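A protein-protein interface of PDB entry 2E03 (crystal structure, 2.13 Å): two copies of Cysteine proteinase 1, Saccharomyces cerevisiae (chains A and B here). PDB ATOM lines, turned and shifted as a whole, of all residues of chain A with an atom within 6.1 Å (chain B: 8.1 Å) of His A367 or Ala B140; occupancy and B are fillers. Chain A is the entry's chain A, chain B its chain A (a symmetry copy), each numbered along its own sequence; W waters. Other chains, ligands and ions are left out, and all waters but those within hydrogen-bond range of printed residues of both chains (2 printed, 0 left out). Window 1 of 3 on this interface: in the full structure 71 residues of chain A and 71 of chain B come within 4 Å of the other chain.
O of Arg A365 is in hydrogen-bond range of NE2 of Gln B136, 3.0 Å away. The side-chain carboxylate (OE2) of Glu A368 is in hydrogen-bond range of the side-chain hydroxyl (OG1) of Thr B186. The guanidinium group (NH1) of Arg B189 lies within salt-bridge range of the side-chain carboxylate (OE1) of Glu A368 (2.9 Å). The backbone carbonyl oxygen (O) of His A367 sits close to the guanidinium group (NH1) of Arg B189 (3.1 Å).
O of Leu B139 lies within hydrogen-bond range of NE of Arg B189, 2.8 Å away. The backbone carbonyl oxygen (O) of Ala B140 is in hydrogen-bond range of the guanidinium group (NH2) of Arg B189, 2.8 Å away. The side-chain amide nitrogen (NE2) of Gln B136 lies within hydrogen-bond range of the backbone carbonyl oxygen (O) of Ile B130. The backbone carbonyl oxygen of Arg A363 lies within hydrogen-bond range of the backbone NH of Glu A368, at 2.9 Å.
Among the printed residues, pairs that only touch across the chains: Tyr A366 with Arg B189 (3.3 Å), His A367 with Gln B136 (3.5 Å), Tyr A366 with Ile B130 (3.5 Å), Arg A365 with Ile B130 (3.6 Å), His A367 with Leu B139 (3.7 Å), His A367 with Ala B140 (3.8 Å) and Tyr A366 with Leu B139 (3.9 Å).
Of the printed residues of chain A, Ala B140 touches His A367. Of the printed residues of chain B, Glu A368 touches Thr B186 and Arg B189. Printed residues of chain B within 4 Å of Arg A365: Ile B130 and Gln B136. Of the printed residues of chain A, Thr B186 touches Glu A368 (2.9 Å). Printed residues of chain A within 4 Å of Leu B139: Tyr A366 and His A367. Of the printed residues of chain A, Arg B189 touches Tyr A366, His A367 and Glu A368. Leu B138 touches none of the printed residues of chain A. Leu B134 touches none of the printed residues of chain A. The nearest residue of chain B that does not touch His A367 is Tyr B137 (5.6 Å). The nearest printed residue of chain B that does not touch Tyr A366 is Gln B136 (4.9 Å).
Hydrophobic or aromatic side chains of chain A that line the printed part of chain B: Tyr A366 and His A367. Of the 17 printed residues of chain B, 6 touch a printed residue of chain A. Hydrophobic or aromatic side chains of chain B that line the printed part of chain A: Ile B130, Leu B139 and Ala B140. Among the printed residues, 11 pairs touch across the chains. Among the printed residues, Asp or Glu carboxylates within 4 Å of a Lys or Arg side-chain nitrogen of the other chain: Glu A368 with Arg B189 (2.9 Å).
No position is printed for both chains. Of the 11 pairs that touch across the chains among the printed residues, none has its exchanged pair printed and touching as well.
Water W1 lies within hydrogen-bond range of O of Glu A368 (2.7 Å) and NH1 of Arg B189 (3.3 Å). Water W2 lies within hydrogen-bond range of the side-chain hydroxyl (OG1) of Thr B186 (2.8 Å), the side-chain carboxylate (OE1) of Glu A368 (3.1 Å) and the guanidinium group (NH1) of Arg B189 (3.3 Å).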
ATOM      1  N   SER A 362      19.458  -5.457  -6.097  1.00  0.00           N
ATOM      2  CA  SER A 362      19.491  -5.940  -4.720  1.00  0.00           C
ATOM      3  C   SER A 362      20.439  -7.130  -4.569  1.00  0.00           C
ATOM      4  O   SER A 362      21.085  -7.294  -3.525  1.00  0.00           O
ATOM      5  CB  SER A 362      18.058  -6.317  -4.256  1.00  0.00           C
ATOM      6  OG  SER A 362      17.306  -5.135  -4.026  1.00  0.00           O
ATOM      7  N   ARG A 363      20.532  -7.971  -5.597  1.00  0.00           N
ATOM      8  CA  ARG A 363      21.468  -9.101  -5.473  1.00  0.00           C
ATOM      9  C   ARG A 363      22.918  -8.506  -5.283  1.00  0.00           C
ATOM     10  O   ARG A 363      23.726  -8.994  -4.496  1.00  0.00           O
ATOM     11  CB  ARG A 363      21.422  -9.946  -6.725  1.00  0.00           C
ATOM     12  CG  ARG A 363      20.356 -11.101  -6.814  1.00  0.00           C
ATOM     13  CD  ARG A 363      20.592 -11.882  -8.143  1.00  0.00           C
ATOM     14  NE  ARG A 363      20.042 -11.140  -9.293  1.00  0.00           N
ATOM     15  CZ  ARG A 363      20.357 -11.333 -10.552  1.00  0.00           C
ATOM     16  NH1 ARG A 363      21.254 -12.228 -10.865  1.00  0.00           N
ATOM     17  NH2 ARG A 363      19.757 -10.705 -11.533  1.00  0.00           N
ATOM     18  N   ILE A 364      23.219  -7.422  -5.998  1.00  0.00           N
ATOM     19  CA  ILE A 364      24.549  -6.792  -5.890  1.00  0.00           C
ATOM     20  C   ILE A 364      24.787  -6.179  -4.546  1.00  0.00           C
ATOM     21  O   ILE A 364      25.812  -6.416  -3.915  1.00  0.00           O
ATOM     22  CB  ILE A 364      24.728  -5.725  -6.947  1.00  0.00           C
ATOM     23  CG1 ILE A 364      24.617  -6.377  -8.319  1.00  0.00           C
ATOM     24  CG2 ILE A 364      26.152  -4.980  -6.746  1.00  0.00           C
ATOM     25  CD1 ILE A 364      24.487  -5.363  -9.427  1.00  0.00           C
ATOM     26  N   ARG A 365      23.809  -5.415  -4.065  1.00  0.00           N
ATOM     27  CA  ARG A 365      23.920  -4.759  -2.769  1.00  0.00           C
ATOM     28  C   ARG A 365      23.974  -5.720  -1.593  1.00  0.00           C
ATOM     29  O   ARG A 365      24.679  -5.467  -0.583  1.00  0.00           O
ATOM     30  CB  ARG A 365      22.730  -3.791  -2.563  1.00  0.00           C
ATOM     31  CG  ARG A 365      22.899  -2.482  -3.322  1.00  0.00           C
ATOM     32  CD  ARG A 365      21.981  -1.379  -2.773  1.00  0.00           C
ATOM     33  NE  ARG A 365      21.047  -0.887  -3.793  1.00  0.00           N
ATOM     34  CZ  ARG A 365      21.222   0.236  -4.460  1.00  0.00           C
ATOM     35  NH1 ARG A 365      22.303   0.984  -4.197  1.00  0.00           N
ATOM     36  NH2 ARG A 365      20.332   0.606  -5.372  1.00  0.00           N
ATOM     37  N   TYR A 366      23.237  -6.836  -1.719  1.00  0.00           N
ATOM     38  CA  TYR A 366      23.166  -7.796  -0.603  1.00  0.00           C
ATOM     39  C   TYR A 366      24.179  -8.916  -0.610  1.00  0.00           C
ATOM     40  O   TYR A 366      23.960  -9.937   0.033  1.00  0.00           O
ATOM     41  CB  TYR A 366      21.740  -8.391  -0.435  1.00  0.00           C
ATOM     42  CG  TYR A 366      20.852  -7.409   0.291  1.00  0.00           C
ATOM     43  CD1 TYR A 366      20.327  -6.327  -0.362  1.00  0.00           C
ATOM     44  CD2 TYR A 366      20.608  -7.537   1.654  1.00  0.00           C
ATOM     45  CE1 TYR A 366      19.563  -5.376   0.327  1.00  0.00           C
ATOM     46  CE2 TYR A 366      19.867  -6.606   2.351  1.00  0.00           C
ATOM     47  CZ  TYR A 366      19.354  -5.521   1.683  1.00  0.00           C
ATOM     48  OH  TYR A 366      18.767  -4.506   2.419  1.00  0.00           O
ATOM     49  N   HIS A 367      25.301  -8.691  -1.308  1.00  0.00           N
ATOM     50  CA  HIS A 367      26.404  -9.657  -1.333  1.00  0.00           C
ATOM     51  C   HIS A 367      26.128 -10.994  -2.074  1.00  0.00           C
ATOM     52  O   HIS A 367      26.831 -11.978  -1.857  1.00  0.00           O
ATOM     53  CB  HIS A 367      26.762  -9.973   0.105  1.00  0.00           C
ATOM     54  CG  HIS A 367      28.218 -10.236   0.342  1.00  0.00           C
ATOM     55  ND1 HIS A 367      28.897 -11.277  -0.267  1.00  0.00           N
ATOM     56  CD2 HIS A 367      29.140  -9.560   1.091  1.00  0.00           C
ATOM     57  CE1 HIS A 367      30.178 -11.223   0.083  1.00  0.00           C
ATOM     58  NE2 HIS A 367      30.351 -10.192   0.903  1.00  0.00           N
ATOM     59  N   GLU A 368      25.118 -11.026  -2.928  1.00  0.00           N
ATOM     60  CA  GLU A 368      24.783 -12.235  -3.641  1.00  0.00           C
ATOM     61  C   GLU A 368      25.403 -12.352  -5.041  1.00  0.00           C
ATOM     62  O   GLU A 368      25.788 -13.431  -5.438  1.00  0.00           O
ATOM     63  CB  GLU A 368      23.270 -12.372  -3.695  1.00  0.00           C
ATOM     64  CG  GLU A 368      22.724 -13.583  -4.425  1.00  0.00           C
ATOM     65  CD  GLU A 368      23.270 -14.942  -3.922  1.00  0.00           C
ATOM     66  OE1 GLU A 368      23.653 -15.107  -2.752  1.00  0.00           O
ATOM     67  OE2 GLU A 368      23.294 -15.873  -4.749  1.00  0.00           O
ATOM     68  N   SER A 369      25.517 -11.262  -5.784  1.00  0.00           N
ATOM     69  CA  SER A 369      26.112 -11.348  -7.114  1.00  0.00           C
ATOM     70  C   SER A 369      27.194 -10.270  -7.324  1.00  0.00           C
ATOM     71  O   SER A 369      27.122  -9.151  -6.768  1.00  0.00           O
ATOM     72  CB  SER A 369      25.035 -11.221  -8.183  1.00  0.00           C
ATOM     73  OG  SER A 369      25.443 -11.861  -9.362  1.00  0.00           O
ATOM     74  N   PHE B 118      21.438 -15.126  12.317  1.00  0.00           N
ATOM     75  CA  PHE B 118      21.644 -14.148  11.266  1.00  0.00           C
ATOM     76  C   PHE B 118      20.407 -13.250  11.083  1.00  0.00           C
ATOM     77  O   PHE B 118      20.543 -12.031  10.893  1.00  0.00           O
ATOM     78  CB  PHE B 118      21.944 -14.885   9.961  1.00  0.00           C
ATOM     79  CG  PHE B 118      21.809 -14.055   8.757  1.00  0.00           C
ATOM     80  CD1 PHE B 118      22.875 -13.270   8.338  1.00  0.00           C
ATOM     81  CD2 PHE B 118      20.616 -14.060   8.012  1.00  0.00           C
ATOM     82  CE1 PHE B 118      22.772 -12.464   7.144  1.00  0.00           C
ATOM     83  CE2 PHE B 118      20.507 -13.266   6.837  1.00  0.00           C
ATOM     84  CZ  PHE B 118      21.593 -12.470   6.404  1.00  0.00           C
ATOM     85  N   ILE B 130      23.171  -0.446   4.131  1.00  0.00           N
ATOM     86  CA  ILE B 130      23.388  -1.769   3.543  1.00  0.00           C
ATOM     87  C   ILE B 130      24.908  -1.989   3.288  1.00  0.00           C
ATOM     88  O   ILE B 130      25.443  -3.053   3.568  1.00  0.00           O
ATOM     89  CB  ILE B 130      22.554  -1.886   2.251  1.00  0.00           C
ATOM     90  CG1 ILE B 130      22.825  -3.233   1.549  1.00  0.00           C
ATOM     91  CG2 ILE B 130      22.891  -0.696   1.323  1.00  0.00           C
ATOM     92  CD1 ILE B 130      22.661  -4.447   2.428  1.00  0.00           C
ATOM     93  N   ARG B 133      30.205  -1.712   7.113  1.00  0.00           N
ATOM     94  CA  ARG B 133      31.128  -2.784   7.376  1.00  0.00           C
ATOM     95  C   ARG B 133      30.458  -3.988   8.059  1.00  0.00           C
ATOM     96  O   ARG B 133      30.686  -5.102   7.655  1.00  0.00           O
ATOM     97  CB  ARG B 133      32.283  -2.284   8.235  1.00  0.00           C
ATOM     98  CG  ARG B 133      33.519  -3.226   8.174  1.00  0.00           C
ATOM     99  CD  ARG B 133      34.663  -2.622   9.057  1.00  0.00           C
ATOM    100  NE  ARG B 133      35.900  -3.385   8.949  1.00  0.00           N
ATOM    101  CZ  ARG B 133      37.011  -3.094   9.622  1.00  0.00           C
ATOM    102  NH1 ARG B 133      37.013  -2.040  10.448  1.00  0.00           N
ATOM    103  NH2 ARG B 133      38.100  -3.840   9.467  1.00  0.00           N
ATOM    104  N   LEU B 134      29.620  -3.754   9.065  1.00  0.00           N
ATOM    105  CA  LEU B 134      28.948  -4.850   9.754  1.00  0.00           C
ATOM    106  C   LEU B 134      27.937  -5.579   8.902  1.00  0.00           C
ATOM    107  O   LEU B 134      27.885  -6.830   8.905  1.00  0.00           O
ATOM    108  CB  LEU B 134      28.195  -4.377  11.025  1.00  0.00           C
ATOM    109  CG  LEU B 134      27.446  -5.565  11.707  1.00  0.00           C
ATOM    110  CD1 LEU B 134      28.441  -6.669  12.204  1.00  0.00           C
ATOM    111  CD2 LEU B 134      26.651  -5.072  12.901  1.00  0.00           C
ATOM    112  N   VAL B 135      27.147  -4.833   8.147  1.00  0.00           N
ATOM    113  CA  VAL B 135      26.080  -5.513   7.439  1.00  0.00           C
ATOM    114  C   VAL B 135      26.613  -6.338   6.289  1.00  0.00           C
ATOM    115  O   VAL B 135      26.164  -7.445   6.072  1.00  0.00           O
ATOM    116  CB  VAL B 135      24.974  -4.522   7.025  1.00  0.00           C
ATOM    117  CG1 VAL B 135      23.902  -5.230   6.175  1.00  0.00           C
ATOM    118  CG2 VAL B 135      24.341  -3.918   8.304  1.00  0.00           C
ATOM    119  N   GLN B 136      27.627  -5.810   5.606  1.00  0.00           N
ATOM    120  CA  GLN B 136      28.276  -6.549   4.531  1.00  0.00           C
ATOM    121  C   GLN B 136      28.926  -7.771   5.155  1.00  0.00           C
ATOM    122  O   GLN B 136      28.875  -8.858   4.590  1.00  0.00           O
ATOM    123  CB  GLN B 136      29.319  -5.676   3.856  1.00  0.00           C
ATOM    124  CG  GLN B 136      28.643  -4.687   2.938  1.00  0.00           C
ATOM    125  CD  GLN B 136      27.832  -5.371   1.831  1.00  0.00           C
ATOM    126  OE1 GLN B 136      28.376  -6.170   1.104  1.00  0.00           O
ATOM    127  NE2 GLN B 136      26.524  -5.052   1.707  1.00  0.00           N
ATOM    128  N   TYR B 137      29.527  -7.598   6.330  1.00  0.00           N
ATOM    129  CA  TYR B 137      30.170  -8.730   6.976  1.00  0.00           C
ATOM    130  C   TYR B 137      29.114  -9.808   7.301  1.00  0.00           C
ATOM    131  O   TYR B 137      29.340 -11.000   7.073  1.00  0.00           O
ATOM    132  CB  TYR B 137      30.858  -8.307   8.280  1.00  0.00           C
ATOM    133  CG  TYR B 137      31.554  -9.455   8.892  1.00  0.00           C
ATOM    134  CD1 TYR B 137      32.776  -9.894   8.389  1.00  0.00           C
ATOM    135  CD2 TYR B 137      30.985 -10.157   9.943  1.00  0.00           C
ATOM    136  CE1 TYR B 137      33.423 -11.018   8.951  1.00  0.00           C
ATOM    137  CE2 TYR B 137      31.599 -11.275  10.480  1.00  0.00           C
ATOM    138  CZ  TYR B 137      32.820 -11.697   9.979  1.00  0.00           C
ATOM    139  OH  TYR B 137      33.409 -12.819  10.496  1.00  0.00           O
ATOM    140  N   LEU B 138      27.986  -9.394   7.883  1.00  0.00           N
ATOM    141  CA  LEU B 138      26.871 -10.330   8.224  1.00  0.00           C
ATOM    142  C   LEU B 138      26.411 -11.117   6.993  1.00  0.00           C
ATOM    143  O   LEU B 138      26.121 -12.334   7.085  1.00  0.00           O
ATOM    144  CB  LEU B 138      25.659  -9.542   8.789  1.00  0.00           C
ATOM    145  CG  LEU B 138      26.000  -9.105  10.212  1.00  0.00           C
ATOM    146  CD1 LEU B 138      24.881  -8.243  10.743  1.00  0.00           C
ATOM    147  CD2 LEU B 138      26.171 -10.368  11.112  1.00  0.00           C
ATOM    148  N   LEU B 139      26.372 -10.437   5.840  1.00  0.00           N
ATOM    149  CA  LEU B 139      25.963 -11.056   4.573  1.00  0.00           C
ATOM    150  C   LEU B 139      27.004 -11.985   3.877  1.00  0.00           C
ATOM    151  O   LEU B 139      26.631 -12.791   3.007  1.00  0.00           O
ATOM    152  CB  LEU B 139      25.559  -9.941   3.594  1.00  0.00           C
ATOM    153  CG  LEU B 139      24.366  -9.074   4.094  1.00  0.00           C
ATOM    154  CD1 LEU B 139      24.184  -7.775   3.231  1.00  0.00           C
ATOM    155  CD2 LEU B 139      23.091  -9.907   3.988  1.00  0.00           C
ATOM    156  N   ALA B 140      28.293 -11.837   4.225  1.00  0.00           N
ATOM    157  CA  ALA B 140      29.345 -12.617   3.584  1.00  0.00           C
ATOM    158  C   ALA B 140      29.241 -14.144   3.690  1.00  0.00           C
ATOM    159  O   ALA B 140      29.284 -14.818   2.679  1.00  0.00           O
ATOM    160  CB  ALA B 140      30.765 -12.159   4.104  1.00  0.00           C
ATOM    161  N   ALA B 141      29.105 -14.677   4.893  1.00  0.00           N
ATOM    162  CA  ALA B 141      29.052 -16.142   5.072  1.00  0.00           C
ATOM    163  C   ALA B 141      28.210 -16.538   6.267  1.00  0.00           C
ATOM    164  O   ALA B 141      28.712 -17.207   7.154  1.00  0.00           O
ATOM    165  CB  ALA B 141      30.508 -16.708   5.274  1.00  0.00           C
ATOM    166  N   PRO B 142      26.905 -16.203   6.269  1.00  0.00           N
ATOM    167  CA  PRO B 142      26.079 -16.567   7.446  1.00  0.00           C
ATOM    168  C   PRO B 142      25.908 -18.022   7.896  1.00  0.00           C
ATOM    169  O   PRO B 142      25.603 -18.276   9.059  1.00  0.00           O
ATOM    170  CB  PRO B 142      24.732 -15.865   7.168  1.00  0.00           C
ATOM    171  CG  PRO B 142      24.643 -15.730   5.668  1.00  0.00           C
ATOM    172  CD  PRO B 142      26.137 -15.478   5.234  1.00  0.00           C
ATOM    173  N   THR B 143      26.117 -18.996   7.022  1.00  0.00           N
ATOM    174  CA  THR B 143      25.899 -20.345   7.489  1.00  0.00           C
ATOM    175  C   THR B 143      27.106 -21.210   7.335  1.00  0.00           C
ATOM    176  O   THR B 143      26.979 -22.367   6.999  1.00  0.00           O
ATOM    177  CB  THR B 143      24.661 -20.977   6.809  1.00  0.00           C
ATOM    178  OG1 THR B 143      24.895 -21.159   5.413  1.00  0.00           O
ATOM    179  CG2 THR B 143      23.506 -20.003   6.910  1.00  0.00           C
ATOM    180  N   GLU B 144      28.277 -20.638   7.614  1.00  0.00           N
ATOM    181  CA  GLU B 144      29.478 -21.425   7.505  1.00  0.00           C
ATOM    182  C   GLU B 144      29.495 -22.458   8.636  1.00  0.00           C
ATOM    183  O   GLU B 144      28.850 -22.280   9.713  1.00  0.00           O
ATOM    184  CB  GLU B 144      30.737 -20.530   7.522  1.00  0.00           C
ATOM    185  CG  GLU B 144      31.039 -19.738   8.820  1.00  0.00           C
ATOM    186  CD  GLU B 144      32.423 -19.006   8.750  1.00  0.00           C
ATOM    187  OE1 GLU B 144      33.305 -19.310   9.603  1.00  0.00           O
ATOM    188  OE2 GLU B 144      32.623 -18.136   7.842  1.00  0.00           O
ATOM    189  N   THR B 185      22.297 -19.711   1.925  1.00  0.00           N
ATOM    190  CA  THR B 185      22.814 -18.344   1.966  1.00  0.00           C
ATOM    191  C   THR B 185      22.166 -17.393   0.992  1.00  0.00           C
ATOM    192  O   THR B 185      21.918 -16.248   1.353  1.00  0.00           O
ATOM    193  CB  THR B 185      24.364 -18.342   1.783  1.00  0.00           C
ATOM    194  OG1 THR B 185      24.911 -19.019   2.915  1.00  0.00           O
ATOM    195  CG2 THR B 185      24.933 -16.865   1.761  1.00  0.00           C
ATOM    196  N   THR B 186      21.870 -17.855  -0.220  1.00  0.00           N
ATOM    197  CA  THR B 186      21.206 -17.008  -1.232  1.00  0.00           C
ATOM    198  C   THR B 186      19.812 -16.597  -0.698  1.00  0.00           C
ATOM    199  O   THR B 186      19.364 -15.462  -0.898  1.00  0.00           O
ATOM    200  CB  THR B 186      21.025 -17.770  -2.551  1.00  0.00           C
ATOM    201  OG1 THR B 186      22.316 -18.051  -3.080  1.00  0.00           O
ATOM    202  CG2 THR B 186      20.262 -16.904  -3.594  1.00  0.00           C
ATOM    203  N   ARG B 189      20.143 -14.067   2.039  1.00  0.00           N
ATOM    204  CA  ARG B 189      20.457 -12.694   1.561  1.00  0.00           C
ATOM    205  C   ARG B 189      19.170 -12.040   1.082  1.00  0.00           C
ATOM    206  O   ARG B 189      18.958 -10.808   1.240  1.00  0.00           O
ATOM    207  CB  ARG B 189      21.566 -12.737   0.457  1.00  0.00           C
ATOM    208  CG  ARG B 189      22.934 -13.046   1.067  1.00  0.00           C
ATOM    209  CD  ARG B 189      24.020 -13.277  -0.001  1.00  0.00           C
ATOM    210  NE  ARG B 189      25.310 -13.560   0.607  1.00  0.00           N
ATOM    211  CZ  ARG B 189      26.254 -14.328   0.033  1.00  0.00           C
ATOM    212  NH1 ARG B 189      26.042 -14.916  -1.145  1.00  0.00           N
ATOM    213  NH2 ARG B 189      27.442 -14.451   0.620  1.00  0.00           N
HETATM  214  O   HOH W   1      26.932 -15.543  -4.255  1.00  0.00           O
HETATM  215  O   HOH W   2      24.889 -17.826  -2.085  1.00  0.00           O
